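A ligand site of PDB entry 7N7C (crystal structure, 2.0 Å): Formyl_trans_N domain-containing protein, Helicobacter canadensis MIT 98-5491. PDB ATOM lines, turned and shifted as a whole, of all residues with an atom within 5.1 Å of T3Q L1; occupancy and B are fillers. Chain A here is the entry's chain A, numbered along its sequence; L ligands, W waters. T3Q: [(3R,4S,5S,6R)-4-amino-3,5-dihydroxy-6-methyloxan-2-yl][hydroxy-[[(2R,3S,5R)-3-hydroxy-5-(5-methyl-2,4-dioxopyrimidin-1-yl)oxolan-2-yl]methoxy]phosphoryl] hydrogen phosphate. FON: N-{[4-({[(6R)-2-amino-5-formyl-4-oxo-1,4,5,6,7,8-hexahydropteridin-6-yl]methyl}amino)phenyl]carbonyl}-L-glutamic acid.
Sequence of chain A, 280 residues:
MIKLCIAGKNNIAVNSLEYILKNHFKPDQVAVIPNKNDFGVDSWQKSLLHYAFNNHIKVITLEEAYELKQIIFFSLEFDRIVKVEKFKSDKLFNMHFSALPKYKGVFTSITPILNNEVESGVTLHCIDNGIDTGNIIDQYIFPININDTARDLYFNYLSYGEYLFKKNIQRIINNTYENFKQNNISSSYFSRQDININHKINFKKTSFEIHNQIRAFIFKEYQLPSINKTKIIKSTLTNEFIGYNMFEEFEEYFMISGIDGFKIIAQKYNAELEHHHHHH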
ATOM      1  N   LYS A   9     -34.422  -4.872  17.324  1.00  0.00           N
ATOM      2  CA  LYS A   9     -34.851  -6.280  17.333  1.00  0.00           C
ATOM      3  C   LYS A   9     -35.571  -6.668  18.623  1.00  0.00           C
ATOM      4  O   LYS A   9     -35.585  -5.864  19.594  1.00  0.00           O
ATOM      5  CB  LYS A   9     -33.629  -7.181  17.128  1.00  0.00           C
ATOM      6  CG  LYS A   9     -32.568  -7.137  18.220  1.00  0.00           C
ATOM      7  CD  LYS A   9     -31.609  -8.330  18.110  1.00  0.00           C
ATOM      8  CE  LYS A   9     -30.480  -8.289  19.121  1.00  0.00           C
ATOM      9  NZ  LYS A   9     -29.560  -9.452  18.998  1.00  0.00           N
ATOM     10  N   ASN A  35     -32.423  -5.513  12.362  1.00  0.00           N
ATOM     11  CA  ASN A  35     -31.027  -5.956  12.524  1.00  0.00           C
ATOM     12  C   ASN A  35     -30.695  -6.910  11.376  1.00  0.00           C
ATOM     13  O   ASN A  35     -31.604  -7.502  10.779  1.00  0.00           O
ATOM     14  CB  ASN A  35     -30.800  -6.554  13.914  1.00  0.00           C
ATOM     15  CG  ASN A  35     -30.645  -5.506  14.999  1.00  0.00           C
ATOM     16  OD1 ASN A  35     -31.021  -4.351  14.788  1.00  0.00           O
ATOM     17  ND2 ASN A  35     -30.109  -5.898  16.152  1.00  0.00           N
ATOM     18  N   GLU A  77     -32.064  -2.077  20.678  1.00  0.00           N
ATOM     19  CA  GLU A  77     -31.127  -3.189  20.386  1.00  0.00           C
ATOM     20  C   GLU A  77     -30.771  -3.173  18.903  1.00  0.00           C
ATOM     21  O   GLU A  77     -30.569  -4.249  18.308  1.00  0.00           O
ATOM     22  CB  GLU A  77     -31.740  -4.523  20.844  1.00  0.00           C
ATOM     23  CG  GLU A  77     -32.019  -4.537  22.335  1.00  0.00           C
ATOM     24  CD  GLU A  77     -30.790  -4.179  23.149  1.00  0.00           C
ATOM     25  OE1 GLU A  77     -29.826  -5.012  23.152  1.00  0.00           O
ATOM     26  OE2 GLU A  77     -30.795  -3.076  23.776  1.00  0.00           O
ATOM     27  N   PHE A  78     -30.571  -1.987  18.353  1.00  0.00           N
ATOM     28  CA  PHE A  78     -30.051  -1.814  16.976  1.00  0.00           C
ATOM     29  C   PHE A  78     -28.582  -2.266  16.956  1.00  0.00           C
ATOM     30  O   PHE A  78     -27.859  -1.984  17.932  1.00  0.00           O
ATOM     31  CB  PHE A  78     -30.276  -0.382  16.502  1.00  0.00           C
ATOM     32  CG  PHE A  78     -30.021  -0.152  15.042  1.00  0.00           C
ATOM     33  CD1 PHE A  78     -30.535  -1.011  14.080  1.00  0.00           C
ATOM     34  CD2 PHE A  78     -29.333   0.971  14.601  1.00  0.00           C
ATOM     35  CE1 PHE A  78     -30.282  -0.788  12.731  1.00  0.00           C
ATOM     36  CE2 PHE A  78     -29.126   1.217  13.251  1.00  0.00           C
ATOM     37  CZ  PHE A  78     -29.608   0.336  12.311  1.00  0.00           C
ATOM     38  N   ASP A  79     -28.157  -2.900  15.862  1.00  0.00           N
ATOM     39  CA  ASP A  79     -26.819  -3.544  15.761  1.00  0.00           C
ATOM     40  C   ASP A  79     -25.778  -2.572  15.162  1.00  0.00           C
ATOM     41  O   ASP A  79     -24.604  -2.947  15.118  1.00  0.00           O
ATOM     42  CB  ASP A  79     -26.907  -4.877  15.006  1.00  0.00           C
ATOM     43  CG  ASP A  79     -27.553  -4.844  13.632  1.00  0.00           C
ATOM     44  OD1 ASP A  79     -28.000  -3.757  13.190  1.00  0.00           O
ATOM     45  OD2 ASP A  79     -27.602  -5.920  12.992  1.00  0.00           O
ATOM     46  N   ASN A  94     -31.982   6.151  22.116  1.00  0.00           N
ATOM     47  CA  ASN A  94     -31.495   4.763  22.316  1.00  0.00           C
ATOM     48  C   ASN A  94     -31.918   4.310  23.709  1.00  0.00           C
ATOM     49  O   ASN A  94     -31.878   5.133  24.666  1.00  0.00           O
ATOM     50  CB  ASN A  94     -29.975   4.621  22.142  1.00  0.00           C
ATOM     51  CG  ASN A  94     -29.568   3.174  22.291  1.00  0.00           C
ATOM     52  OD1 ASN A  94     -30.088   2.332  21.569  1.00  0.00           O
ATOM     53  ND2 ASN A  94     -28.748   2.866  23.284  1.00  0.00           N
ATOM     54  N   MET A  95     -32.334   3.058  23.798  1.00  0.00           N
ATOM     55  CA  MET A  95     -32.496   2.340  25.071  1.00  0.00           C
ATOM     56  C   MET A  95     -31.292   1.387  25.196  1.00  0.00           C
ATOM     57  O   MET A  95     -31.142   0.494  24.345  1.00  0.00           O
ATOM     58  CB  MET A  95     -33.808   1.542  25.066  1.00  0.00           C
ATOM     59  CG  MET A  95     -34.130   1.001  26.409  1.00  0.00           C
ATOM     60  SD  MET A  95     -34.615   2.296  27.554  1.00  0.00           S
ATOM     61  CE  MET A  95     -36.205   2.778  26.896  1.00  0.00           C
ATOM     62  N   HIS A  96     -30.458   1.636  26.194  1.00  0.00           N
ATOM     63  CA  HIS A  96     -29.250   0.840  26.519  1.00  0.00           C
ATOM     64  C   HIS A  96     -29.533  -0.020  27.753  1.00  0.00           C
ATOM     65  O   HIS A  96     -30.111   0.491  28.756  1.00  0.00           O
ATOM     66  CB  HIS A  96     -28.039   1.756  26.692  1.00  0.00           C
ATOM     67  CG  HIS A  96     -26.818   0.980  27.045  1.00  0.00           C
ATOM     68  ND1 HIS A  96     -26.197   0.131  26.158  1.00  0.00           N
ATOM     69  CD2 HIS A  96     -26.165   0.820  28.214  1.00  0.00           C
ATOM     70  CE1 HIS A  96     -25.194  -0.473  26.755  1.00  0.00           C
ATOM     71  NE2 HIS A  96     -25.140  -0.057  27.989  1.00  0.00           N
ATOM     72  N   GLY A 105     -21.195  -0.348  26.088  1.00  0.00           N
ATOM     73  CA  GLY A 105     -20.606  -1.397  25.240  1.00  0.00           C
ATOM     74  C   GLY A 105     -21.559  -2.561  25.126  1.00  0.00           C
ATOM     75  O   GLY A 105     -22.765  -2.319  25.068  1.00  0.00           O
ATOM     76  N   VAL A 106     -21.047  -3.794  25.122  1.00  0.00           N
ATOM     77  CA  VAL A 106     -21.855  -4.956  24.682  1.00  0.00           C
ATOM     78  C   VAL A 106     -21.865  -6.002  25.784  1.00  0.00           C
ATOM     79  O   VAL A 106     -21.184  -5.829  26.837  1.00  0.00           O
ATOM     80  CB  VAL A 106     -21.345  -5.492  23.331  1.00  0.00           C
ATOM     81  CG1 VAL A 106     -21.317  -4.402  22.273  1.00  0.00           C
ATOM     82  CG2 VAL A 106     -19.965  -6.105  23.477  1.00  0.00           C
ATOM     83  N   PHE A 107     -22.651  -7.044  25.570  1.00  0.00           N
ATOM     84  CA  PHE A 107     -22.738  -8.230  26.450  1.00  0.00           C
ATOM     85  C   PHE A 107     -23.215  -7.793  27.834  1.00  0.00           C
ATOM     86  O   PHE A 107     -22.697  -8.325  28.815  1.00  0.00           O
ATOM     87  CB  PHE A 107     -21.368  -8.912  26.515  1.00  0.00           C
ATOM     88  CG  PHE A 107     -21.011  -9.789  25.335  1.00  0.00           C
ATOM     89  CD1 PHE A 107     -21.922 -10.656  24.776  1.00  0.00           C
ATOM     90  CD2 PHE A 107     -19.714  -9.828  24.848  1.00  0.00           C
ATOM     91  CE1 PHE A 107     -21.564 -11.501  23.723  1.00  0.00           C
ATOM     92  CE2 PHE A 107     -19.363 -10.681  23.797  1.00  0.00           C
ATOM     93  CZ  PHE A 107     -20.289 -11.533  23.256  1.00  0.00           C
ATOM     94  N   THR A 108     -24.122  -6.810  27.941  1.00  0.00           N
ATOM     95  CA  THR A 108     -24.461  -6.173  29.244  1.00  0.00           C
ATOM     96  C   THR A 108     -25.280  -7.121  30.138  1.00  0.00           C
ATOM     97  O   THR A 108     -25.584  -6.719  31.271  1.00  0.00           O
ATOM     98  CB  THR A 108     -25.237  -4.857  29.091  1.00  0.00           C
ATOM     99  OG1 THR A 108     -26.485  -5.060  28.428  1.00  0.00           O
ATOM    100  CG2 THR A 108     -24.413  -3.837  28.349  1.00  0.00           C
ATOM    101  N   SER A 109     -25.670  -8.292  29.630  1.00  0.00           N
ATOM    102  CA  SER A 109     -26.330  -9.360  30.405  1.00  0.00           C
ATOM    103  C   SER A 109     -25.269 -10.258  31.061  1.00  0.00           C
ATOM    104  O   SER A 109     -25.603 -10.957  31.991  1.00  0.00           O
ATOM    105  CB  SER A 109     -27.270 -10.139  29.512  1.00  0.00           C
ATOM    106  OG  SER A 109     -28.454  -9.400  29.274  1.00  0.00           O
ATOM    107  N   ILE A 110     -24.019 -10.193  30.592  1.00  0.00           N
ATOM    108  CA  ILE A 110     -22.841 -10.903  31.148  1.00  0.00           C
ATOM    109  C   ILE A 110     -22.058  -9.975  32.116  1.00  0.00           C
ATOM    110  O   ILE A 110     -21.739 -10.401  33.267  1.00  0.00           O
ATOM    111  CB  ILE A 110     -21.983 -11.430  29.991  1.00  0.00           C
ATOM    112  CG1 ILE A 110     -22.813 -12.316  29.049  1.00  0.00           C
ATOM    113  CG2 ILE A 110     -20.742 -12.145  30.507  1.00  0.00           C
ATOM    114  CD1 ILE A 110     -22.029 -13.132  28.054  1.00  0.00           C
ATOM    115  N   ASP A 132     -22.812   4.705  23.696  1.00  0.00           N
ATOM    116  CA  ASP A 132     -23.671   4.701  24.916  1.00  0.00           C
ATOM    117  C   ASP A 132     -23.281   5.867  25.818  1.00  0.00           C
ATOM    118  O   ASP A 132     -23.486   5.756  27.049  1.00  0.00           O
ATOM    119  CB  ASP A 132     -23.603   3.355  25.643  1.00  0.00           C
ATOM    120  CG  ASP A 132     -23.968   2.119  24.840  1.00  0.00           C
ATOM    121  OD1 ASP A 132     -25.085   2.039  24.229  1.00  0.00           O
ATOM    122  OD2 ASP A 132     -23.185   1.161  24.925  1.00  0.00           O
ATOM    123  N   TYR A 154     -31.165 -10.616  30.780  1.00  0.00           N
ATOM    124  CA  TYR A 154     -31.556 -10.125  29.429  1.00  0.00           C
ATOM    125  C   TYR A 154     -33.080  -9.969  29.339  1.00  0.00           C
ATOM    126  O   TYR A 154     -33.526  -8.919  28.831  1.00  0.00           O
ATOM    127  CB  TYR A 154     -31.075 -11.062  28.335  1.00  0.00           C
ATOM    128  CG  TYR A 154     -31.326 -10.494  26.961  1.00  0.00           C
ATOM    129  CD1 TYR A 154     -30.584  -9.419  26.485  1.00  0.00           C
ATOM    130  CD2 TYR A 154     -32.330 -11.003  26.153  1.00  0.00           C
ATOM    131  CE1 TYR A 154     -30.812  -8.888  25.236  1.00  0.00           C
ATOM    132  CE2 TYR A 154     -32.542 -10.502  24.877  1.00  0.00           C
ATOM    133  CZ  TYR A 154     -31.784  -9.439  24.413  1.00  0.00           C
ATOM    134  OH  TYR A 154     -32.033  -8.901  23.184  1.00  0.00           O
ATOM    135  N   ARG A 192     -16.639  -6.415  22.521  1.00  0.00           N
ATOM    136  CA  ARG A 192     -16.765  -7.874  22.258  1.00  0.00           C
ATOM    137  C   ARG A 192     -15.446  -8.568  22.648  1.00  0.00           C
ATOM    138  O   ARG A 192     -15.519  -9.674  23.205  1.00  0.00           O
ATOM    139  CB  ARG A 192     -17.212  -8.164  20.813  1.00  0.00           C
ATOM    140  CG  ARG A 192     -18.554  -7.512  20.449  1.00  0.00           C
ATOM    141  CD  ARG A 192     -19.607  -8.366  19.740  1.00  0.00           C
ATOM    142  NE  ARG A 192     -20.973  -8.323  20.318  1.00  0.00           N
ATOM    143  CZ  ARG A 192     -21.969  -7.522  19.947  1.00  0.00           C
ATOM    144  NH1 ARG A 192     -21.787  -6.631  18.984  1.00  0.00           N
ATOM    145  NH2 ARG A 192     -23.160  -7.627  20.552  1.00  0.00           N
ATOM    146  N   ILE A 197     -16.445 -15.865  25.705  1.00  0.00           N
ATOM    147  CA  ILE A 197     -17.679 -16.700  25.946  1.00  0.00           C
ATOM    148  C   ILE A 197     -17.307 -18.131  26.356  1.00  0.00           C
ATOM    149  O   ILE A 197     -18.210 -18.860  26.818  1.00  0.00           O
ATOM    150  CB  ILE A 197     -18.619 -16.719  24.717  1.00  0.00           C
ATOM    151  CG1 ILE A 197     -17.897 -17.156  23.439  1.00  0.00           C
ATOM    152  CG2 ILE A 197     -19.295 -15.357  24.545  1.00  0.00           C
ATOM    153  CD1 ILE A 197     -18.617 -18.213  22.629  1.00  0.00           C
ATOM    154  N   PHE A 219     -26.814 -18.937  28.907  1.00  0.00           N
ATOM    155  CA  PHE A 219     -27.819 -18.355  27.991  1.00  0.00           C
ATOM    156  C   PHE A 219     -27.971 -19.327  26.825  1.00  0.00           C
ATOM    157  O   PHE A 219     -27.236 -19.144  25.866  1.00  0.00           O
ATOM    158  CB  PHE A 219     -27.339 -16.982  27.511  1.00  0.00           C
ATOM    159  CG  PHE A 219     -28.413 -16.051  27.002  1.00  0.00           C
ATOM    160  CD1 PHE A 219     -29.455 -16.525  26.221  1.00  0.00           C
ATOM    161  CD2 PHE A 219     -28.345 -14.701  27.261  1.00  0.00           C
ATOM    162  CE1 PHE A 219     -30.427 -15.655  25.759  1.00  0.00           C
ATOM    163  CE2 PHE A 219     -29.323 -13.837  26.810  1.00  0.00           C
ATOM    164  CZ  PHE A 219     -30.357 -14.314  26.049  1.00  0.00           C
ATOM    165  N   TYR A 222     -27.331 -19.150  23.072  1.00  0.00           N
ATOM    166  CA  TYR A 222     -25.984 -18.747  22.615  1.00  0.00           C
ATOM    167  C   TYR A 222     -24.976 -19.819  23.043  1.00  0.00           C
ATOM    168  O   TYR A 222     -24.311 -20.366  22.175  1.00  0.00           O
ATOM    169  CB  TYR A 222     -25.629 -17.343  23.122  1.00  0.00           C
ATOM    170  CG  TYR A 222     -26.423 -16.214  22.500  1.00  0.00           C
ATOM    171  CD1 TYR A 222     -26.219 -15.804  21.198  1.00  0.00           C
ATOM    172  CD2 TYR A 222     -27.385 -15.542  23.236  1.00  0.00           C
ATOM    173  CE1 TYR A 222     -26.923 -14.749  20.645  1.00  0.00           C
ATOM    174  CE2 TYR A 222     -28.138 -14.499  22.686  1.00  0.00           C
ATOM    175  CZ  TYR A 222     -27.896 -14.105  21.385  1.00  0.00           C
ATOM    176  OH  TYR A 222     -28.617 -13.087  20.837  1.00  0.00           O
ATOM    177  N   GLN A 223     -24.862 -20.083  24.349  1.00  0.00           N
ATOM    178  CA  GLN A 223     -23.888 -21.072  24.887  1.00  0.00           C
ATOM    179  C   GLN A 223     -24.292 -21.430  26.328  1.00  0.00           C
ATOM    180  O   GLN A 223     -25.176 -20.736  26.938  1.00  0.00           O
ATOM    181  CB  GLN A 223     -22.440 -20.543  24.855  1.00  0.00           C
ATOM    182  CG  GLN A 223     -22.128 -19.548  25.995  1.00  0.00           C
ATOM    183  CD  GLN A 223     -22.715 -18.177  25.759  1.00  0.00           C
ATOM    184  OE1 GLN A 223     -22.431 -17.571  24.722  1.00  0.00           O
ATOM    185  NE2 GLN A 223     -23.520 -17.688  26.699  1.00  0.00           N
HETATM  186  O4  T3Q L   1     -22.472 -15.000  21.969  1.00  0.00           O
HETATM  187  C4  T3Q L   1     -23.291 -14.516  22.717  1.00  0.00           C
HETATM  188  N3  T3Q L   1     -23.461 -15.005  23.939  1.00  0.00           N
HETATM  189  C2  T3Q L   1     -24.351 -14.490  24.775  1.00  0.00           C
HETATM  190  O2  T3Q L   1     -24.441 -14.972  25.863  1.00  0.00           O
HETATM  191  C5  T3Q L   1     -24.081 -13.469  22.339  1.00  0.00           C
HETATM  192  C5M T3Q L   1     -23.934 -12.893  20.985  1.00  0.00           C
HETATM  193  C6  T3Q L   1     -24.986 -12.935  23.223  1.00  0.00           C
HETATM  194  N1  T3Q L   1     -25.144 -13.412  24.413  1.00  0.00           N
HETATM  195  C1' T3Q L   1     -26.092 -12.863  25.337  1.00  0.00           C
HETATM  196  O4' T3Q L   1     -27.178 -12.216  24.756  1.00  0.00           O
HETATM  197  C2' T3Q L   1     -25.403 -11.824  26.200  1.00  0.00           C
HETATM  198  C3' T3Q L   1     -25.859 -10.517  25.637  1.00  0.00           C
HETATM  199  O3' T3Q L   1     -25.851  -9.476  26.595  1.00  0.00           O
HETATM  200  C4' T3Q L   1     -27.226 -10.870  25.139  1.00  0.00           C
HETATM  201  C5' T3Q L   1     -27.646 -10.004  23.990  1.00  0.00           C
HETATM  202  O5' T3Q L   1     -26.798 -10.162  22.913  1.00  0.00           O
HETATM  203  PA  T3Q L   1     -26.718  -9.105  21.828  1.00  0.00           P
HETATM  204  O1A T3Q L   1     -27.944  -9.049  21.200  1.00  0.00           O
HETATM  205  O2A T3Q L   1     -25.657  -9.375  20.954  1.00  0.00           O
HETATM  206  O3A T3Q L   1     -26.611  -7.750  22.570  1.00  0.00           O
HETATM  207  PB  T3Q L   1     -25.482  -7.182  23.488  1.00  0.00           P
HETATM  208  O1B T3Q L   1     -24.192  -7.630  23.068  1.00  0.00           O
HETATM  209  O2B T3Q L   1     -25.822  -7.386  24.845  1.00  0.00           O
HETATM  210  O3B T3Q L   1     -25.663  -5.614  23.288  1.00  0.00           O
HETATM  211  O4Q T3Q L   1     -28.144  -3.151  20.086  1.00  0.00           O
HETATM  212  C4Q T3Q L   1     -26.906  -3.531  20.596  1.00  0.00           C
HETATM  213  C5Q T3Q L   1     -26.816  -5.033  20.668  1.00  0.00           C
HETATM  214  O5Q T3Q L   1     -25.472  -5.344  21.006  1.00  0.00           O
HETATM  215  C6Q T3Q L   1     -27.260  -5.677  19.373  1.00  0.00           C
HETATM  216  C3Q T3Q L   1     -26.825  -3.044  22.012  1.00  0.00           C
HETATM  217  N3Q T3Q L   1     -27.182  -1.633  22.140  1.00  0.00           N
HETATM  218  C2Q T3Q L   1     -25.408  -3.331  22.456  1.00  0.00           C
HETATM  219  O2Q T3Q L   1     -25.296  -3.007  23.812  1.00  0.00           O
HETATM  220  C1Q T3Q L   1     -25.080  -4.823  22.238  1.00  0.00           C
HETATM  221  N1  FON L   2     -25.079   4.905  17.679  1.00  0.00           N
HETATM  222  C2  FON L   2     -24.284   5.769  18.372  1.00  0.00           C
HETATM  223  NA2 FON L   2     -23.643   6.724  17.693  1.00  0.00           N
HETATM  224  N3  FON L   2     -24.194   5.720  19.699  1.00  0.00           N
HETATM  225  C4  FON L   2     -24.874   4.734  20.404  1.00  0.00           C
HETATM  226  O4  FON L   2     -24.736   4.735  21.622  1.00  0.00           O
HETATM  227  C4A FON L   2     -25.724   3.801  19.721  1.00  0.00           C
HETATM  228  N5  FON L   2     -26.377   2.679  20.353  1.00  0.00           N
HETATM  229  C6  FON L   2     -26.850   1.598  19.410  1.00  0.00           C
HETATM  230  C7  FON L   2     -27.544   2.238  18.217  1.00  0.00           C
HETATM  231  N8  FON L   2     -26.608   3.118  17.562  1.00  0.00           N
HETATM  232  C8A FON L   2     -25.806   3.932  18.312  1.00  0.00           C
HETATM  233  C9  FON L   2     -25.706   0.707  18.872  1.00  0.00           C
HETATM  234  N10 FON L   2     -24.883  -0.005  19.840  1.00  0.00           N
HETATM  235  C11 FON L   2     -21.309  -1.886  18.740  1.00  0.00           C
HETATM  236  C12 FON L   2     -22.326  -1.643  17.819  1.00  0.00           C
HETATM  237  C13 FON L   2     -23.506  -1.044  18.196  1.00  0.00           C
HETATM  238  C14 FON L   2     -23.698  -0.626  19.506  1.00  0.00           C
HETATM  239  C15 FON L   2     -22.683  -0.854  20.434  1.00  0.00           C
HETATM  240  C16 FON L   2     -21.509  -1.460  20.058  1.00  0.00           C
HETATM  241  C   FON L   2     -20.065  -2.534  18.206  1.00  0.00           C
HETATM  242  O   FON L   2     -19.998  -2.870  17.029  1.00  0.00           O
HETATM  243  N   FON L   2     -19.039  -2.691  19.064  1.00  0.00           N
HETATM  244  CA  FON L   2     -17.715  -3.188  18.670  1.00  0.00           C
HETATM  245  CB  FON L   2     -16.645  -2.079  18.698  1.00  0.00           C
HETATM  246  CG  FON L   2     -16.590  -1.220  17.449  1.00  0.00           C
HETATM  247  CD  FON L   2     -15.789   0.055  17.662  1.00  0.00           C
HETATM  248  OE1 FON L   2     -14.828   0.005  18.466  1.00  0.00           O
HETATM  249  OE2 FON L   2     -16.166   1.106  17.102  1.00  0.00           O
HETATM  250  CT  FON L   2     -17.267  -4.281  19.658  1.00  0.00           C
HETATM  251  O1  FON L   2     -17.736  -4.234  20.802  1.00  0.00           O
HETATM  252  O2  FON L   2     -16.380  -5.058  19.281  1.00  0.00           O
HETATM  253  CP1 FON L   2     -26.487   2.327  21.685  1.00  0.00           C
HETATM  254  O3  FON L   2     -26.533   1.127  22.102  1.00  0.00           O
HETATM  255  O   HOH W   1     -29.876  -0.619  21.987  1.00  0.00           O
HETATM  256  O   HOH W   2     -28.625  -2.589  25.036  1.00  0.00           O
HETATM  257  O   HOH W   3     -23.695  -5.100  18.552  1.00  0.00           O
HETATM  258  O   HOH W   4     -20.582 -14.071  20.126  1.00  0.00           O
HETATM  259  O   HOH W   5     -27.856  -7.238  27.503  1.00  0.00           O
HETATM  260  O   HOH W   6     -21.650 -18.048  22.398  1.00  0.00           O
HETATM  261  O   HOH W   7     -24.189  -0.359  23.064  1.00  0.00           O
HETATM  262  O   HOH W   8     -30.175  -7.506  22.117  1.00  0.00           O
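The guanidinium group of Arg 192 lies within salt-bridge range of an oxygen (O1B) of T3Q L1 (2.7 Å). The backbone NH of Asp 132 sits at hydrogen-bond distance from an oxygen (O4) of FON L2 (2.8 Å). The backbone NH (N) of Phe 107 sits at hydrogen-bond distance from an oxygen (O1B) of T3Q L1 (3.0 Å). O3' of T3Q L1 sits at hydrogen-bond distance from N of Thr 108 (3.5 Å). The side-chain amide oxygen (OE1) of Gln 223 sits at hydrogen-bond distance from a nitrogen (N3) of T3Q L1, 2.9 Å away. An oxygen (O1) of FON L2 lies within hydrogen-bond range of the backbone NH (N) of Arg 192 (3.0 Å). The side-chain carboxylate of Asp 132 sits close to an oxygen (O3) of FON L2 (2.7 Å). O of Phe 78 is in hydrogen-bond range of O4Q of T3Q L1, at 2.5 Å. An oxygen (O2Q) of T3Q L1 is in hydrogen-bond range of the backbone carbonyl oxygen of Gly 105. The side-chain amide nitrogen of Asn 94 lies close to an oxygen (O3) of FON L2, 3.1 Å away. O4Q of T3Q L1 sits close to O of Glu 77 (3.2 Å). The backbone NH of Ser 109 sits at hydrogen-bond distance from an oxygen (O3') of T3Q L1, 3.3 Å away. The backbone NH of Phe 78 sits at hydrogen-bond distance from an oxygen (O4Q) of T3Q L1 (3.2 Å). NZ of Lys 9 lies within salt-bridge range of O1A of T3Q L1 (2.8 Å).
N3Q of T3Q L1 sits at hydrogen-bond distance from O3 of FON L2, 2.8 Å away.
ND1 of His 96 lies within hydrogen-bond range of OD1 of Asp 132. O of Glu 77 sits at hydrogen-bond distance from ND2 of Asn 35 (2.8 Å). N of Gly 105 sits at hydrogen-bond distance from OD2 of Asp 132. OG of Ser 109 sits close to N of Tyr 154, at 3.3 Å.
Residues that only touch T3Q L1: His 96, Val 106, Ile 110, Tyr 154, Phe 219 and Tyr 222. The nearest printed residue that does not touch T3Q L1 is Ile 197 (4.1 Å).
Water W8 lies within hydrogen-bond range of OH of Tyr 154, OE1 of Glu 77 and O1A of T3Q L1. Water W1 lies within hydrogen-bond range of N3Q of T3Q L1 (2.9 Å), O of Met 95 (2.9 Å), N of Glu 77 (2.9 Å) and OD1 of Asn 94 (3.0 Å). Water W3 lies within hydrogen-bond range of the guanidinium group (NH1) of Arg 192 (2.5 Å) and an oxygen (O5Q) of T3Q L1 (3.0 Å). Water W5 lies within hydrogen-bond range of the side-chain hydroxyl (OG1) of Thr 108, the side-chain hydroxyl (OG) of Ser 109 and an oxygen (O3') of T3Q L1. Water W6 bridges OE1 of Gln 223 and O4 of T3Q L1. Water W2 lies within hydrogen-bond range of OE2 of Glu 77 (2.6 Å) and N3Q of T3Q L1 (3.4 Å).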
